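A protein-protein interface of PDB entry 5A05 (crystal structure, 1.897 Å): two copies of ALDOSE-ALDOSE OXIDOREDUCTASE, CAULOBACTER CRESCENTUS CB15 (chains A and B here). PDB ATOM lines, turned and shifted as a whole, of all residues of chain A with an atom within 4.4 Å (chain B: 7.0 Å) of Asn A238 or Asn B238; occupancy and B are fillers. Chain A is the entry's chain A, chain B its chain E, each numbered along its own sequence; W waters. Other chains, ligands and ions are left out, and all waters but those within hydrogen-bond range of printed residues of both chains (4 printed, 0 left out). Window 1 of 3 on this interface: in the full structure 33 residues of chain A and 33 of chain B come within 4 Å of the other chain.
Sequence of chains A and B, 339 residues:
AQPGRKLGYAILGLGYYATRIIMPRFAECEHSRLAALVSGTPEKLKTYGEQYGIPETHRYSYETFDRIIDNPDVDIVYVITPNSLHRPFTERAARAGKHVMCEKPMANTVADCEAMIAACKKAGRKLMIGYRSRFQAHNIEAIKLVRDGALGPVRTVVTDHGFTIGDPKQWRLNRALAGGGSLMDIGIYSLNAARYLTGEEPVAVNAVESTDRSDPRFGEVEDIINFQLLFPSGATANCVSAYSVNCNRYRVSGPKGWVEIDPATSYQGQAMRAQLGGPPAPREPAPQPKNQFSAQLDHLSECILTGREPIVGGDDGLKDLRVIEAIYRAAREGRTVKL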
ATOM      1  N   VAL A 157     -14.607  -6.757  29.287  1.00  0.00           N
ATOM      2  CA  VAL A 157     -15.695  -6.300  30.139  1.00  0.00           C
ATOM      3  C   VAL A 157     -16.921  -7.096  29.725  1.00  0.00           C
ATOM      4  O   VAL A 157     -17.272  -7.131  28.555  1.00  0.00           O
ATOM      5  CB  VAL A 157     -15.978  -4.795  29.990  1.00  0.00           C
ATOM      6  CG1 VAL A 157     -17.201  -4.378  30.855  1.00  0.00           C
ATOM      7  CG2 VAL A 157     -14.734  -3.974  30.356  1.00  0.00           C
ATOM      8  N   VAL A 158     -17.549  -7.771  30.679  1.00  0.00           N
ATOM      9  CA  VAL A 158     -18.760  -8.509  30.395  1.00  0.00           C
ATOM     10  C   VAL A 158     -19.841  -7.899  31.262  1.00  0.00           C
ATOM     11  O   VAL A 158     -19.741  -7.918  32.495  1.00  0.00           O
ATOM     12  CB  VAL A 158     -18.594 -10.017  30.686  1.00  0.00           C
ATOM     13  CG1 VAL A 158     -19.895 -10.756  30.461  1.00  0.00           C
ATOM     14  CG2 VAL A 158     -17.473 -10.609  29.831  1.00  0.00           C
ATOM     15  N   THR A 159     -20.865  -7.326  30.646  1.00  0.00           N
ATOM     16  CA  THR A 159     -21.841  -6.591  31.444  1.00  0.00           C
ATOM     17  C   THR A 159     -23.245  -6.803  30.904  1.00  0.00           C
ATOM     18  O   THR A 159     -23.470  -6.734  29.688  1.00  0.00           O
ATOM     19  CB  THR A 159     -21.489  -5.084  31.488  1.00  0.00           C
ATOM     20  OG1 THR A 159     -22.527  -4.358  32.163  1.00  0.00           O
ATOM     21  CG2 THR A 159     -21.277  -4.511  30.070  1.00  0.00           C
ATOM     22  N   ASN A 226     -27.997  -7.386  22.082  1.00  0.00           N
ATOM     23  CA  ASN A 226     -26.708  -7.613  22.726  1.00  0.00           C
ATOM     24  C   ASN A 226     -25.638  -7.096  21.804  1.00  0.00           C
ATOM     25  O   ASN A 226     -25.802  -7.153  20.591  1.00  0.00           O
ATOM     26  CB  ASN A 226     -26.484  -9.096  23.020  1.00  0.00           C
ATOM     27  CG  ASN A 226     -27.556  -9.670  23.912  1.00  0.00           C
ATOM     28  OD1 ASN A 226     -28.171  -8.941  24.689  1.00  0.00           O
ATOM     29  ND2 ASN A 226     -27.810 -10.976  23.786  1.00  0.00           N
ATOM     30  N   PHE A 227     -24.546  -6.588  22.360  1.00  0.00           N
ATOM     31  CA  PHE A 227     -23.544  -5.997  21.492  1.00  0.00           C
ATOM     32  C   PHE A 227     -22.120  -6.263  21.970  1.00  0.00           C
ATOM     33  O   PHE A 227     -21.890  -6.590  23.138  1.00  0.00           O
ATOM     34  CB  PHE A 227     -23.805  -4.481  21.322  1.00  0.00           C
ATOM     35  CG  PHE A 227     -23.997  -3.713  22.616  1.00  0.00           C
ATOM     36  CD1 PHE A 227     -25.236  -3.699  23.265  1.00  0.00           C
ATOM     37  CD2 PHE A 227     -22.962  -2.954  23.144  1.00  0.00           C
ATOM     38  CE1 PHE A 227     -25.424  -2.963  24.430  1.00  0.00           C
ATOM     39  CE2 PHE A 227     -23.139  -2.212  24.319  1.00  0.00           C
ATOM     40  CZ  PHE A 227     -24.375  -2.218  24.959  1.00  0.00           C
ATOM     41  N   GLN A 228     -21.187  -6.182  21.023  1.00  0.00           N
ATOM     42  CA  GLN A 228     -19.760  -6.300  21.300  1.00  0.00           C
ATOM     43  C   GLN A 228     -19.075  -4.995  20.942  1.00  0.00           C
ATOM     44  O   GLN A 228     -19.442  -4.345  19.960  1.00  0.00           O
ATOM     45  CB  GLN A 228     -19.121  -7.432  20.498  1.00  0.00           C
ATOM     46  CG  GLN A 228     -19.842  -8.754  20.571  1.00  0.00           C
ATOM     47  CD  GLN A 228     -19.107  -9.826  19.812  1.00  0.00           C
ATOM     48  OE1 GLN A 228     -19.044  -9.794  18.581  1.00  0.00           O
ATOM     49  NE2 GLN A 228     -18.518 -10.772  20.537  1.00  0.00           N
ATOM     50  N   ALA A 237     -15.592  -5.721  24.925  1.00  0.00           N
ATOM     51  CA  ALA A 237     -16.751  -5.818  25.804  1.00  0.00           C
ATOM     52  C   ALA A 237     -17.852  -6.670  25.164  1.00  0.00           C
ATOM     53  O   ALA A 237     -18.107  -6.558  23.958  1.00  0.00           O
ATOM     54  CB  ALA A 237     -17.279  -4.415  26.147  1.00  0.00           C
ATOM     55  N   ASN A 238     -18.453  -7.550  25.963  1.00  0.00           N
ATOM     56  CA  ASN A 238     -19.666  -8.296  25.595  1.00  0.00           C
ATOM     57  C   ASN A 238     -20.779  -7.742  26.461  1.00  0.00           C
ATOM     58  O   ASN A 238     -20.668  -7.778  27.690  1.00  0.00           O
ATOM     59  CB  ASN A 238     -19.534  -9.804  25.854  1.00  0.00           C
ATOM     60  CG  ASN A 238     -19.018 -10.583  24.657  1.00  0.00           C
ATOM     61  OD1 ASN A 238     -18.705 -10.025  23.605  1.00  0.00           O
ATOM     62  ND2 ASN A 238     -18.915 -11.902  24.828  1.00  0.00           N
ATOM     63  N   CYS A 239     -21.839  -7.227  25.846  1.00  0.00           N
ATOM     64  CA  CYS A 239     -22.880  -6.539  26.600  1.00  0.00           C
ATOM     65  C   CYS A 239     -24.259  -7.091  26.294  1.00  0.00           C
ATOM     66  O   CYS A 239     -24.572  -7.325  25.131  1.00  0.00           O
ATOM     67  CB  CYS A 239     -22.869  -5.042  26.286  1.00  0.00           C
ATOM     68  SG  CYS A 239     -21.256  -4.197  26.471  1.00  0.00           S
ATOM     69  N   VAL A 240     -25.071  -7.281  27.335  1.00  0.00           N
ATOM     70  CA  VAL A 240     -26.496  -7.616  27.181  1.00  0.00           C
ATOM     71  C   VAL A 240     -27.375  -6.407  27.507  1.00  0.00           C
ATOM     72  O   VAL A 240     -27.104  -5.661  28.453  1.00  0.00           O
ATOM     73  CB  VAL A 240     -26.902  -8.817  28.078  1.00  0.00           C
ATOM     74  CG1 VAL A 240     -28.430  -8.935  28.227  1.00  0.00           C
ATOM     75  CG2 VAL A 240     -26.319 -10.111  27.519  1.00  0.00           C
ATOM     76  N   THR B 156     -31.260 -15.426  27.263  1.00  0.00           N
ATOM     77  CA  THR B 156     -29.829 -15.160  27.148  1.00  0.00           C
ATOM     78  C   THR B 156     -28.991 -16.224  27.839  1.00  0.00           C
ATOM     79  O   THR B 156     -29.375 -16.765  28.881  1.00  0.00           O
ATOM     80  CB  THR B 156     -29.437 -13.798  27.765  1.00  0.00           C
ATOM     81  OG1 THR B 156     -29.681 -13.832  29.180  1.00  0.00           O
ATOM     82  CG2 THR B 156     -30.230 -12.631  27.134  1.00  0.00           C
ATOM     83  N   VAL B 157     -27.840 -16.503  27.239  1.00  0.00           N
ATOM     84  CA  VAL B 157     -26.771 -17.249  27.875  1.00  0.00           C
ATOM     85  C   VAL B 157     -25.524 -16.373  27.834  1.00  0.00           C
ATOM     86  O   VAL B 157     -25.134 -15.904  26.778  1.00  0.00           O
ATOM     87  CB  VAL B 157     -26.496 -18.592  27.175  1.00  0.00           C
ATOM     88  CG1 VAL B 157     -25.286 -19.283  27.806  1.00  0.00           C
ATOM     89  CG2 VAL B 157     -27.732 -19.493  27.262  1.00  0.00           C
ATOM     90  N   VAL B 158     -24.912 -16.127  28.986  1.00  0.00           N
ATOM     91  CA  VAL B 158     -23.714 -15.309  29.035  1.00  0.00           C
ATOM     92  C   VAL B 158     -22.632 -16.177  29.652  1.00  0.00           C
ATOM     93  O   VAL B 158     -22.766 -16.619  30.788  1.00  0.00           O
ATOM     94  CB  VAL B 158     -23.925 -14.020  29.853  1.00  0.00           C
ATOM     95  CG1 VAL B 158     -22.611 -13.268  30.023  1.00  0.00           C
ATOM     96  CG2 VAL B 158     -24.995 -13.126  29.193  1.00  0.00           C
ATOM     97  N   THR B 159     -21.581 -16.471  28.897  1.00  0.00           N
ATOM     98  CA  THR B 159     -20.625 -17.468  29.360  1.00  0.00           C
ATOM     99  C   THR B 159     -19.206 -17.078  28.965  1.00  0.00           C
ATOM    100  O   THR B 159     -18.958 -16.648  27.830  1.00  0.00           O
ATOM    101  CB  THR B 159     -21.001 -18.881  28.820  1.00  0.00           C
ATOM    102  OG1 THR B 159     -20.003 -19.844  29.183  1.00  0.00           O
ATOM    103  CG2 THR B 159     -21.185 -18.878  27.307  1.00  0.00           C
ATOM    104  N   ASP B 160     -18.279 -17.212  29.916  1.00  0.00           N
ATOM    105  CA  ASP B 160     -16.898 -16.798  29.712  1.00  0.00           C
ATOM    106  C   ASP B 160     -15.957 -17.927  30.084  1.00  0.00           C
ATOM    107  O   ASP B 160     -16.031 -18.454  31.190  1.00  0.00           O
ATOM    108  CB  ASP B 160     -16.533 -15.572  30.560  1.00  0.00           C
ATOM    109  CG  ASP B 160     -17.540 -14.453  30.464  1.00  0.00           C
ATOM    110  OD1 ASP B 160     -18.182 -14.284  29.392  1.00  0.00           O
ATOM    111  OD2 ASP B 160     -17.669 -13.712  31.479  1.00  0.00           O
ATOM    112  N   SER B 190     -17.546 -22.428  26.299  1.00  0.00           N
ATOM    113  CA  SER B 190     -18.607 -21.410  26.175  1.00  0.00           C
ATOM    114  C   SER B 190     -19.613 -21.796  25.096  1.00  0.00           C
ATOM    115  O   SER B 190     -20.839 -21.699  25.277  1.00  0.00           O
ATOM    116  CB  SER B 190     -18.013 -20.038  25.842  1.00  0.00           C
ATOM    117  OG  SER B 190     -17.164 -19.563  26.885  1.00  0.00           O
ATOM    118  N   ALA B 194     -23.511 -22.962  25.566  1.00  0.00           N
ATOM    119  CA  ALA B 194     -24.597 -22.249  24.882  1.00  0.00           C
ATOM    120  C   ALA B 194     -25.537 -23.233  24.202  1.00  0.00           C
ATOM    121  O   ALA B 194     -26.759 -23.078  24.252  1.00  0.00           O
ATOM    122  CB  ALA B 194     -24.044 -21.262  23.848  1.00  0.00           C
ATOM    123  N   VAL B 208     -15.586 -10.948  17.602  1.00  0.00           N
ATOM    124  CA  VAL B 208     -14.548  -9.922  17.702  1.00  0.00           C
ATOM    125  C   VAL B 208     -13.284 -10.608  18.198  1.00  0.00           C
ATOM    126  O   VAL B 208     -13.314 -11.292  19.220  1.00  0.00           O
ATOM    127  CB  VAL B 208     -14.933  -8.780  18.686  1.00  0.00           C
ATOM    128  CG1 VAL B 208     -13.744  -7.843  18.927  1.00  0.00           C
ATOM    129  CG2 VAL B 208     -16.152  -8.002  18.180  1.00  0.00           C
ATOM    130  N   ILE B 225     -11.154 -14.155  21.512  1.00  0.00           N
ATOM    131  CA  ILE B 225     -12.143 -14.066  20.448  1.00  0.00           C
ATOM    132  C   ILE B 225     -13.517 -14.250  21.073  1.00  0.00           C
ATOM    133  O   ILE B 225     -13.882 -15.329  21.549  1.00  0.00           O
ATOM    134  CB  ILE B 225     -11.885 -15.079  19.296  1.00  0.00           C
ATOM    135  CG1 ILE B 225     -12.962 -14.957  18.209  1.00  0.00           C
ATOM    136  CG2 ILE B 225     -11.706 -16.516  19.810  1.00  0.00           C
ATOM    137  CD1 ILE B 225     -12.531 -15.538  16.855  1.00  0.00           C
ATOM    138  N   ASN B 226     -14.255 -13.154  21.120  1.00  0.00           N
ATOM    139  CA  ASN B 226     -15.563 -13.162  21.754  1.00  0.00           C
ATOM    140  C   ASN B 226     -16.619 -13.279  20.685  1.00  0.00           C
ATOM    141  O   ASN B 226     -16.441 -12.747  19.590  1.00  0.00           O
ATOM    142  CB  ASN B 226     -15.756 -11.899  22.585  1.00  0.00           C
ATOM    143  CG  ASN B 226     -14.716 -11.772  23.693  1.00  0.00           C
ATOM    144  OD1 ASN B 226     -14.172 -12.777  24.178  1.00  0.00           O
ATOM    145  ND2 ASN B 226     -14.417 -10.536  24.084  1.00  0.00           N
ATOM    146  N   PHE B 227     -17.706 -13.983  20.978  1.00  0.00           N
ATOM    147  CA  PHE B 227     -18.697 -14.212  19.946  1.00  0.00           C
ATOM    148  C   PHE B 227     -20.140 -14.144  20.446  1.00  0.00           C
ATOM    149  O   PHE B 227     -20.433 -14.314  21.637  1.00  0.00           O
ATOM    150  CB  PHE B 227     -18.431 -15.566  19.226  1.00  0.00           C
ATOM    151  CG  PHE B 227     -18.265 -16.761  20.149  1.00  0.00           C
ATOM    152  CD1 PHE B 227     -17.056 -17.000  20.801  1.00  0.00           C
ATOM    153  CD2 PHE B 227     -19.297 -17.674  20.306  1.00  0.00           C
ATOM    154  CE1 PHE B 227     -16.896 -18.111  21.607  1.00  0.00           C
ATOM    155  CE2 PHE B 227     -19.154 -18.787  21.126  1.00  0.00           C
ATOM    156  CZ  PHE B 227     -17.949 -19.009  21.774  1.00  0.00           C
ATOM    157  N   GLN B 228     -21.033 -13.873  19.501  1.00  0.00           N
ATOM    158  CA  GLN B 228     -22.456 -13.839  19.767  1.00  0.00           C
ATOM    159  C   GLN B 228     -23.145 -14.903  18.958  1.00  0.00           C
ATOM    160  O   GLN B 228     -22.784 -15.135  17.803  1.00  0.00           O
ATOM    161  CB  GLN B 228     -23.042 -12.486  19.412  1.00  0.00           C
ATOM    162  CG  GLN B 228     -22.285 -11.311  19.963  1.00  0.00           C
ATOM    163  CD  GLN B 228     -23.055 -10.031  19.705  1.00  0.00           C
ATOM    164  OE1 GLN B 228     -23.073  -9.533  18.585  1.00  0.00           O
ATOM    165  NE2 GLN B 228     -23.725  -9.516  20.732  1.00  0.00           N
ATOM    166  N   LEU B 229     -24.146 -15.535  19.557  1.00  0.00           N
ATOM    167  CA  LEU B 229     -24.931 -16.554  18.875  1.00  0.00           C
ATOM    168  C   LEU B 229     -26.401 -16.187  18.912  1.00  0.00           C
ATOM    169  O   LEU B 229     -26.900 -15.720  19.940  1.00  0.00           O
ATOM    170  CB  LEU B 229     -24.738 -17.925  19.534  1.00  0.00           C
ATOM    171  CG  LEU B 229     -23.316 -18.474  19.646  1.00  0.00           C
ATOM    172  CD1 LEU B 229     -23.308 -19.828  20.399  1.00  0.00           C
ATOM    173  CD2 LEU B 229     -22.702 -18.634  18.271  1.00  0.00           C
ATOM    174  N   THR B 236     -30.414 -15.958  22.757  1.00  0.00           N
ATOM    175  CA  THR B 236     -29.125 -15.367  22.396  1.00  0.00           C
ATOM    176  C   THR B 236     -28.029 -15.829  23.339  1.00  0.00           C
ATOM    177  O   THR B 236     -28.302 -16.196  24.480  1.00  0.00           O
ATOM    178  CB  THR B 236     -29.164 -13.826  22.445  1.00  0.00           C
ATOM    179  OG1 THR B 236     -29.494 -13.401  23.780  1.00  0.00           O
ATOM    180  CG2 THR B 236     -30.188 -13.286  21.466  1.00  0.00           C
ATOM    181  N   ALA B 237     -26.787 -15.801  22.867  1.00  0.00           N
ATOM    182  CA  ALA B 237     -25.639 -16.014  23.742  1.00  0.00           C
ATOM    183  C   ALA B 237     -24.540 -15.004  23.457  1.00  0.00           C
ATOM    184  O   ALA B 237     -24.296 -14.641  22.300  1.00  0.00           O
ATOM    185  CB  ALA B 237     -25.092 -17.433  23.602  1.00  0.00           C
ATOM    186  N   ASN B 238     -23.904 -14.553  24.536  1.00  0.00           N
ATOM    187  CA  ASN B 238     -22.708 -13.723  24.506  1.00  0.00           C
ATOM    188  C   ASN B 238     -21.608 -14.547  25.140  1.00  0.00           C
ATOM    189  O   ASN B 238     -21.753 -14.961  26.302  1.00  0.00           O
ATOM    190  CB  ASN B 238     -22.887 -12.436  25.315  1.00  0.00           C
ATOM    191  CG  ASN B 238     -23.323 -11.263  24.488  1.00  0.00           C
ATOM    192  OD1 ASN B 238     -23.588 -11.376  23.288  1.00  0.00           O
ATOM    193  ND2 ASN B 238     -23.405 -10.104  25.136  1.00  0.00           N
ATOM    194  N   CYS B 239     -20.515 -14.767  24.413  1.00  0.00           N
ATOM    195  CA  CYS B 239     -19.468 -15.685  24.862  1.00  0.00           C
ATOM    196  C   CYS B 239     -18.080 -15.062  24.823  1.00  0.00           C
ATOM    197  O   CYS B 239     -17.725 -14.386  23.854  1.00  0.00           O
ATOM    198  CB  CYS B 239     -19.455 -16.950  23.994  1.00  0.00           C
ATOM    199  SG  CYS B 239     -21.082 -17.773  23.812  1.00  0.00           S
ATOM    200  N   VAL B 240     -17.291 -15.329  25.864  1.00  0.00           N
ATOM    201  CA  VAL B 240     -15.878 -14.964  25.884  1.00  0.00           C
ATOM    202  C   VAL B 240     -15.009 -16.214  25.762  1.00  0.00           C
ATOM    203  O   VAL B 240     -15.303 -17.247  26.360  1.00  0.00           O
ATOM    204  CB  VAL B 240     -15.493 -14.209  27.178  1.00  0.00           C
ATOM    205  CG1 VAL B 240     -13.971 -14.128  27.336  1.00  0.00           C
ATOM    206  CG2 VAL B 240     -16.077 -12.821  27.163  1.00  0.00           C
ATOM    207  N   SER B 241     -13.959 -16.102  24.954  1.00  0.00           N
ATOM    208  CA  SER B 241     -12.900 -17.094  24.847  1.00  0.00           C
ATOM    209  C   SER B 241     -11.585 -16.341  24.995  1.00  0.00           C
ATOM    210  O   SER B 241     -11.339 -15.411  24.234  1.00  0.00           O
ATOM    211  CB  SER B 241     -12.956 -17.814  23.488  1.00  0.00           C
ATOM    212  OG  SER B 241     -11.883 -18.735  23.346  1.00  0.00           O
HETATM  213  O   HOH W   1     -25.904 -12.318  21.884  1.00  0.00           O
HETATM  214  O   HOH W   2     -19.724 -13.085  27.402  1.00  0.00           O
HETATM  215  O   HOH W   3     -16.398  -8.616  22.743  1.00  0.00           O
HETATM  216  O   HOH W   4     -22.624 -10.009  28.018  1.00  0.00           O
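Water W2 lies within hydrogen-bond range of OD1 of Asp B160, ND2 of Asn A238 and O of Asn B238. Water W3 lies within hydrogen-bond range of OD1 of Asn A238 (2.8 Å), O of Ala A237 (2.9 Å) and ND2 of Asn B226 (3.1 Å). Water W1 lies within hydrogen-bond range of O of Ala B237, OD1 of Asn B238 and ND2 of Asn A226. Water W4 lies within hydrogen-bond range of the backbone carbonyl oxygen (O) of Asn A238 (3.0 Å) and the side-chain amide nitrogen (ND2) of Asn B238 (3.0 Å).
Asn A238 touches four residues of chain B. Of the printed residues of chain A, Cys B239 touches Asn A238 (2.9 Å). Printed residues of chain B within 4 Å of Cys A239: Asn B238 (3.0 Å). Printed residues of chain A within 4 Å of Val B158: Val A158 and Val A240. Of the printed residues of chain A, Phe B227 touches Gln A228 (3.3 Å). Of the printed residues of chain B, Val A158 touches Val B158 (3.7 Å), Asp B160 (3.5 Å) and Val B240 (3.7 Å). The nearest residue of chain B that does not touch Asn A238 is Phe B227 (4.3 Å).
Among the printed residues, merely in contact across the chains: Val A158 with Val B158 (3.7 Å), Val A158 with Asp B160 (3.5 Å), Val A158 with Val B240 (3.7 Å), Asn A226 with Asn B238 (3.7 Å), Gln A228 with Val B208 (3.4 Å), Gln A228 with Gln B228 (3.5 Å), Asn A238 with Asn B226 (3.6 Å), Asn A238 with Asn B238 (3.8 Å), Asn A238 with Val B240 (3.8 Å), Val A240 with Val B158 (3.7 Å) and Val A240 with Asn B238 (3.8 Å).
Val A158 touches its own counterpart, Val B158. Asn A226 touches Gln B228, and with the chains exchanged Gln A228 touches Asn B226. Gln B228 touches its own counterpart, Gln A228. Asn A238 touches Val B240, and with the chains exchanged Val A240 touches Asn B238. 10 positions are printed for both chains.
O of Thr B159 lies within hydrogen-bond range of N of Val B240 (2.9 Å). The backbone carbonyl oxygen of Val A157 lies within hydrogen-bond range of the backbone NH of Asn A238 (2.9 Å). N of Val B157 lies within hydrogen-bond range of O of Thr B236. The backbone NH of Thr A159 sits at hydrogen-bond distance from the backbone carbonyl oxygen of Asn A238 (3.0 Å). The backbone carbonyl oxygen of Asn B226 sits at hydrogen-bond distance from the backbone NH of Val B208, at 2.8 Å. The side-chain amide nitrogen of Gln A228 is in hydrogen-bond range of the side-chain amide oxygen of Asn A238 (3.2 Å).
Of the 19 printed residues of chain B, 10 touch a printed residue of chain A. Printed residues of chain B that touch a printed residue of chain A: Val B158, Asp B160, Val B208, Asn B226, Phe B227, Gln B228, Thr B236, Asn B238, Cys B239 and Val B240. Hydrophobic or aromatic side chains of chain B within 4 Å of the printed part of chain A: Val B158, Val B208 and Val B240. Along chain B the printed residues that touch a printed residue of chain A span positions 158 to 240. Of the 10 printed residues of chain A, 7 touch a printed residue of chain B. Printed residues of chain A that touch a printed residue of chain B: Val A158, Asn A226, Phe A227, Gln A228, Asn A238, Cys A239 and Val A240. Hydrophobic or aromatic side chains of chain A that line the printed part of chain B: Val A158 and Val A240. Among the printed residues, 18 pairs touch across the chains.
NE2 of Gln A228 is in hydrogen-bond range of O of Asn B226, at 3.0 Å. ND2 of Asn A226 is in hydrogen-bond range of OG1 of Thr B236, 3.0 Å away. The side-chain amide nitrogen of Asn B238 lies within hydrogen-bond range of the backbone carbonyl oxygen of Cys A239 (3.0 Å). NE2 of Gln B228 is in hydrogen-bond range of O of Asn A226. N of Phe B227 sits close to NE2 of Gln A228 (3.3 Å). NE2 of Gln B228 lies close to N of Phe A227. ND2 of Asn A238 is in hydrogen-bond range of O of Cys B239 (2.9 Å).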
